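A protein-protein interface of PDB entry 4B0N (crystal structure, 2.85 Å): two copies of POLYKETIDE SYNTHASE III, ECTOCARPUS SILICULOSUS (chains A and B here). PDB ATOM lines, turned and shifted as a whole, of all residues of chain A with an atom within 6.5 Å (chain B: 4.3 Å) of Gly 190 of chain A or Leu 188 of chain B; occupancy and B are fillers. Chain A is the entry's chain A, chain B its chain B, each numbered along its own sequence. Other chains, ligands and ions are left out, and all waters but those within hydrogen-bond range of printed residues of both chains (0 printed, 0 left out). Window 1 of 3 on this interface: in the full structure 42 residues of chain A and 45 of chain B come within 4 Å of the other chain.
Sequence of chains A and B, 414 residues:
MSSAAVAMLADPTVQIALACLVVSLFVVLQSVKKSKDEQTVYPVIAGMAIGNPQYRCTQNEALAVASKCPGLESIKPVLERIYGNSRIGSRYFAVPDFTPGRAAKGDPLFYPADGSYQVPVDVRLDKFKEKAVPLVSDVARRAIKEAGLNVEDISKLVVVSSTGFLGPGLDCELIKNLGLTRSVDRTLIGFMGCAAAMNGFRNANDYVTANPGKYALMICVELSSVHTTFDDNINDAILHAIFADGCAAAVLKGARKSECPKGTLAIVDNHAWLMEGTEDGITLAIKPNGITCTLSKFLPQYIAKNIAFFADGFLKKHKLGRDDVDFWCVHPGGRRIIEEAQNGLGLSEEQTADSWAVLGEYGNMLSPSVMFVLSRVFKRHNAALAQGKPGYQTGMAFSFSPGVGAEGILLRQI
The backbone carbonyl oxygen (O) of Leu 188 of chain A sits at hydrogen-bond distance from the backbone NH (N) of Gly 190 of chain B (3.2 Å). SD of Met 192 of chain A is in hydrogen-bond range of N of Leu 188 of chain B, at 3.3 Å. N of Gly 190 of chain A sits at hydrogen-bond distance from O of Leu 188 of chain B (3.3 Å).
The backbone carbonyl oxygen (O) of Val 159 of chain A is in hydrogen-bond range of the backbone NH (N) of Ile 189 of chain A, at 2.9 Å. The backbone NH of Val 159 of chain B sits at hydrogen-bond distance from the backbone carbonyl oxygen of Thr 187 of chain B. The side-chain sulfur (SD) of Met 192 of chain A sits close to the side-chain amide oxygen (OD1) of Asn 199 of chain A (3.7 Å). The side-chain hydroxyl (OG) of Ser 162 of chain A sits at hydrogen-bond distance from the backbone NH (N) of Met 192 of chain A (3.2 Å). O of Val 159 of chain B lies within hydrogen-bond range of N of Ile 189 of chain B (3.1 Å). The backbone NH of Ser 161 of chain A is in hydrogen-bond range of the backbone carbonyl oxygen of Ile 189 of chain A, 3.1 Å away.
O of Leu 188 of chain B touches O of Leu 188 of chain A, 3.97 Å away. O of Leu 188 of chain A touches CA of Ile 189 of chain B, at 3.5 Å. Ile 189 of chain A touches Leu 188 of chain B. Asp 171 of chain B touches Met 192 of chain A (OD2 to CE, 3.7 Å). Met 192 of chain A touches Thr 187 of chain B (SD to CA, 3.8 Å).
Leu 188 of chain B touches just these residues of chain A: Leu 188 (3.97 Å), Ile 189 (3.6 Å), Gly 190 (3.3 Å) and Met 192 (3.3 Å). Of the printed residues of chain A, Asp 171 of chain B touches Met 192. Printed residues of chain A within 4 Å of Ile 189 of chain B: Leu 188. Printed residues of chain B within 4 Å of Leu 188 of chain A: Leu 188, Ile 189 and Gly 190. Of the printed residues of chain A, Gly 190 of chain B touches Leu 188. Ser 162 of chain A touches none of the printed residues of chain B. Ser 161 of chain A touches none of the printed residues of chain B. The nearest printed residue of chain B that does not touch Gly 190 of chain A is Gly 190 of chain B (4.3 Å).
Of the 6 printed residues of chain B, 5 touch a printed residue of chain A. Printed residues of chain B that touch a printed residue of chain A: Asp 171, Thr 187, Leu 188, Ile 189 and Gly 190. Hydrophobic or aromatic side chains of chain B within 4 Å of the printed part of chain A: Leu 188 and Ile 189. Printed residues of chain A that touch a printed residue of chain B: Leu 188, Ile 189, Gly 190 and Met 192.
Leu 188 of chain A touches its own counterpart, Leu 188 of chain B. Leu 188 of chain A touches Ile 189 of chain B, and with the chains exchanged Ile 189 of chain A touches Leu 188 of chain B. Leu 188 of chain A touches Gly 190 of chain B, and with the chains exchanged Gly 190 of chain A touches Leu 188 of chain B. Of the 8 pairs that touch across the chains among the printed residues, 5 have their exchanged pair printed and touching as well.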
ATOM      1  N   VAL A 159      -5.278  11.508  16.367  1.00  0.00           N
ATOM      2  CA  VAL A 159      -5.309  12.561  17.380  1.00  0.00           C
ATOM      3  C   VAL A 159      -3.923  12.699  18.002  1.00  0.00           C
ATOM      4  O   VAL A 159      -3.255  11.703  18.280  1.00  0.00           O
ATOM      5  CB  VAL A 159      -6.372  12.286  18.469  1.00  0.00           C
ATOM      6  CG1 VAL A 159      -6.319  13.336  19.572  1.00  0.00           C
ATOM      7  CG2 VAL A 159      -7.766  12.232  17.858  1.00  0.00           C
ATOM      8  N   VAL A 160      -3.500  13.943  18.205  1.00  0.00           N
ATOM      9  CA  VAL A 160      -2.179  14.253  18.744  1.00  0.00           C
ATOM     10  C   VAL A 160      -2.305  15.183  19.952  1.00  0.00           C
ATOM     11  O   VAL A 160      -2.935  16.241  19.863  1.00  0.00           O
ATOM     12  CB  VAL A 160      -1.285  14.909  17.668  1.00  0.00           C
ATOM     13  CG1 VAL A 160      -0.031  15.507  18.288  1.00  0.00           C
ATOM     14  CG2 VAL A 160      -0.916  13.906  16.585  1.00  0.00           C
ATOM     15  N   SER A 161      -1.712  14.780  21.077  1.00  0.00           N
ATOM     16  CA  SER A 161      -1.681  15.613  22.281  1.00  0.00           C
ATOM     17  C   SER A 161      -0.610  15.174  23.274  1.00  0.00           C
ATOM     18  O   SER A 161      -0.372  13.983  23.458  1.00  0.00           O
ATOM     19  CB  SER A 161      -3.046  15.628  22.978  1.00  0.00           C
ATOM     20  OG  SER A 161      -3.116  16.686  23.918  1.00  0.00           O
ATOM     21  N   SER A 162       0.030  16.159  23.902  1.00  0.00           N
ATOM     22  CA  SER A 162       0.960  15.933  25.005  1.00  0.00           C
ATOM     23  C   SER A 162       0.378  16.489  26.310  1.00  0.00           C
ATOM     24  O   SER A 162       1.006  16.408  27.368  1.00  0.00           O
ATOM     25  CB  SER A 162       2.313  16.591  24.709  1.00  0.00           C
ATOM     26  OG  SER A 162       2.946  15.997  23.592  1.00  0.00           O
ATOM     27  N   GLY A 164      -3.047  15.798  27.113  1.00  0.00           N
ATOM     28  CA  GLY A 164      -4.232  14.999  27.405  1.00  0.00           C
ATOM     29  C   GLY A 164      -4.066  13.517  27.133  1.00  0.00           C
ATOM     30  O   GLY A 164      -3.570  13.121  26.077  1.00  0.00           O
ATOM     31  N   PHE A 165      -4.471  12.704  28.106  1.00  0.00           N
ATOM     32  CA  PHE A 165      -4.481  11.251  27.973  1.00  0.00           C
ATOM     33  C   PHE A 165      -5.769  10.760  28.604  1.00  0.00           C
ATOM     34  O   PHE A 165      -6.012  10.988  29.792  1.00  0.00           O
ATOM     35  CB  PHE A 165      -3.266  10.618  28.662  1.00  0.00           C
ATOM     36  CG  PHE A 165      -1.945  11.077  28.112  1.00  0.00           C
ATOM     37  CD1 PHE A 165      -1.388  10.460  26.996  1.00  0.00           C
ATOM     38  CD2 PHE A 165      -1.255  12.126  28.708  1.00  0.00           C
ATOM     39  CE1 PHE A 165      -0.170  10.882  26.483  1.00  0.00           C
ATOM     40  CE2 PHE A 165      -0.038  12.555  28.200  1.00  0.00           C
ATOM     41  CZ  PHE A 165       0.505  11.931  27.088  1.00  0.00           C
ATOM     42  N   LEU A 188      -3.609   7.287  18.465  1.00  0.00           N
ATOM     43  CA  LEU A 188      -3.335   8.349  19.421  1.00  0.00           C
ATOM     44  C   LEU A 188      -1.826   8.541  19.616  1.00  0.00           C
ATOM     45  O   LEU A 188      -1.146   7.683  20.194  1.00  0.00           O
ATOM     46  CB  LEU A 188      -4.029   8.061  20.757  1.00  0.00           C
ATOM     47  CG  LEU A 188      -5.562   7.956  20.768  1.00  0.00           C
ATOM     48  CD1 LEU A 188      -6.048   7.268  22.035  1.00  0.00           C
ATOM     49  CD2 LEU A 188      -6.224   9.316  20.615  1.00  0.00           C
ATOM     50  N   ILE A 189      -1.315   9.662  19.107  1.00  0.00           N
ATOM     51  CA  ILE A 189       0.090  10.037  19.269  1.00  0.00           C
ATOM     52  C   ILE A 189       0.223  10.948  20.484  1.00  0.00           C
ATOM     53  O   ILE A 189      -0.234  12.092  20.468  1.00  0.00           O
ATOM     54  CB  ILE A 189       0.654  10.747  18.014  1.00  0.00           C
ATOM     55  CG1 ILE A 189       0.557   9.837  16.785  1.00  0.00           C
ATOM     56  CG2 ILE A 189       2.098  11.189  18.245  1.00  0.00           C
ATOM     57  CD1 ILE A 189       0.940  10.517  15.484  1.00  0.00           C
ATOM     58  N   GLY A 190       0.856  10.431  21.533  1.00  0.00           N
ATOM     59  CA  GLY A 190       0.952  11.141  22.804  1.00  0.00           C
ATOM     60  C   GLY A 190       2.361  11.447  23.278  1.00  0.00           C
ATOM     61  O   GLY A 190       3.302  10.690  23.008  1.00  0.00           O
ATOM     62  N   PHE A 191       2.494  12.578  23.972  1.00  0.00           N
ATOM     63  CA  PHE A 191       3.722  12.970  24.670  1.00  0.00           C
ATOM     64  C   PHE A 191       4.942  13.098  23.744  1.00  0.00           C
ATOM     65  O   PHE A 191       6.074  12.794  24.145  1.00  0.00           O
ATOM     66  CB  PHE A 191       3.996  11.993  25.824  1.00  0.00           C
ATOM     67  CG  PHE A 191       4.309  12.656  27.138  1.00  0.00           C
ATOM     68  CD1 PHE A 191       3.446  13.602  27.687  1.00  0.00           C
ATOM     69  CD2 PHE A 191       5.447  12.300  27.853  1.00  0.00           C
ATOM     70  CE1 PHE A 191       3.726  14.201  28.904  1.00  0.00           C
ATOM     71  CE2 PHE A 191       5.731  12.891  29.072  1.00  0.00           C
ATOM     72  CZ  PHE A 191       4.869  13.844  29.599  1.00  0.00           C
ATOM     73  N   MET A 192       4.707  13.551  22.513  1.00  0.00           N
ATOM     74  CA  MET A 192       5.794  13.798  21.558  1.00  0.00           C
ATOM     75  C   MET A 192       6.107  15.289  21.402  1.00  0.00           C
ATOM     76  O   MET A 192       6.740  15.705  20.430  1.00  0.00           O
ATOM     77  CB  MET A 192       5.499  13.155  20.198  1.00  0.00           C
ATOM     78  CG  MET A 192       5.549  11.634  20.201  1.00  0.00           C
ATOM     79  SD  MET A 192       5.892  10.910  18.583  1.00  0.00           S
ATOM     80  CE  MET A 192       7.668  11.117  18.484  1.00  0.00           C
ATOM     81  N   GLY A 193       5.651  16.083  22.370  1.00  0.00           N
ATOM     82  CA  GLY A 193       6.020  17.492  22.478  1.00  0.00           C
ATOM     83  C   GLY A 193       5.439  18.438  21.444  1.00  0.00           C
ATOM     84  O   GLY A 193       4.324  18.243  20.956  1.00  0.00           O
ATOM     85  N   ASN A 199       4.815  14.438  13.157  1.00  0.00           N
ATOM     86  CA  ASN A 199       4.659  12.994  13.318  1.00  0.00           C
ATOM     87  C   ASN A 199       3.286  12.549  12.841  1.00  0.00           C
ATOM     88  O   ASN A 199       3.151  11.514  12.188  1.00  0.00           O
ATOM     89  CB  ASN A 199       4.880  12.576  14.775  1.00  0.00           C
ATOM     90  CG  ASN A 199       6.239  12.994  15.305  1.00  0.00           C
ATOM     91  OD1 ASN A 199       7.165  12.190  15.372  1.00  0.00           O
ATOM     92  ND2 ASN A 199       6.368  14.263  15.672  1.00  0.00           N
ATOM     93  N   VAL B 159       7.060   2.977  18.937  1.00  0.00           N
ATOM     94  CA  VAL B 159       7.085   2.464  20.306  1.00  0.00           C
ATOM     95  C   VAL B 159       5.694   2.624  20.914  1.00  0.00           C
ATOM     96  O   VAL B 159       5.119   3.714  20.892  1.00  0.00           O
ATOM     97  CB  VAL B 159       8.158   3.165  21.172  1.00  0.00           C
ATOM     98  CG1 VAL B 159       8.192   2.581  22.577  1.00  0.00           C
ATOM     99  CG2 VAL B 159       9.530   3.046  20.523  1.00  0.00           C
ATOM    100  N   ASP B 171      11.763   5.941  22.186  1.00  0.00           N
ATOM    101  CA  ASP B 171      12.175   6.130  20.803  1.00  0.00           C
ATOM    102  C   ASP B 171      13.567   6.759  20.729  1.00  0.00           C
ATOM    103  O   ASP B 171      14.409   6.298  19.963  1.00  0.00           O
ATOM    104  CB  ASP B 171      11.137   6.943  20.005  1.00  0.00           C
ATOM    105  CG  ASP B 171      10.928   8.352  20.547  1.00  0.00           C
ATOM    106  OD1 ASP B 171      11.041   8.557  21.769  1.00  0.00           O
ATOM    107  OD2 ASP B 171      10.637   9.261  19.742  1.00  0.00           O
ATOM    108  N   THR B 187       7.408   7.580  16.084  1.00  0.00           N
ATOM    109  CA  THR B 187       6.020   7.669  16.523  1.00  0.00           C
ATOM    110  C   THR B 187       5.886   6.989  17.879  1.00  0.00           C
ATOM    111  O   THR B 187       6.336   5.853  18.068  1.00  0.00           O
ATOM    112  CB  THR B 187       5.043   7.016  15.519  1.00  0.00           C
ATOM    113  OG1 THR B 187       5.290   7.520  14.202  1.00  0.00           O
ATOM    114  CG2 THR B 187       3.596   7.317  15.902  1.00  0.00           C
ATOM    115  N   LEU B 188       5.280   7.696  18.825  1.00  0.00           N
ATOM    116  CA  LEU B 188       4.997   7.126  20.132  1.00  0.00           C
ATOM    117  C   LEU B 188       3.490   6.996  20.304  1.00  0.00           C
ATOM    118  O   LEU B 188       2.798   7.977  20.581  1.00  0.00           O
ATOM    119  CB  LEU B 188       5.630   7.971  21.245  1.00  0.00           C
ATOM    120  CG  LEU B 188       7.166   8.028  21.259  1.00  0.00           C
ATOM    121  CD1 LEU B 188       7.686   9.254  21.990  1.00  0.00           C
ATOM    122  CD2 LEU B 188       7.775   6.765  21.847  1.00  0.00           C
ATOM    123  N   ILE B 189       2.987   5.782  20.096  1.00  0.00           N
ATOM    124  CA  ILE B 189       1.565   5.491  20.247  1.00  0.00           C
ATOM    125  C   ILE B 189       1.285   5.230  21.724  1.00  0.00           C
ATOM    126  O   ILE B 189       1.650   4.182  22.271  1.00  0.00           O
ATOM    127  CB  ILE B 189       1.120   4.305  19.364  1.00  0.00           C
ATOM    128  CG1 ILE B 189       1.325   4.643  17.884  1.00  0.00           C
ATOM    129  CG2 ILE B 189      -0.337   3.945  19.629  1.00  0.00           C
ATOM    130  CD1 ILE B 189       1.110   3.478  16.943  1.00  0.00           C
ATOM    131  N   GLY B 190       0.648   6.203  22.365  1.00  0.00           N
ATOM    132  CA  GLY B 190       0.461   6.165  23.805  1.00  0.00           C
ATOM    133  C   GLY B 190      -0.979   6.036  24.245  1.00  0.00           C
ATOM    134  O   GLY B 190      -1.862   6.697  23.697  1.00  0.00           O
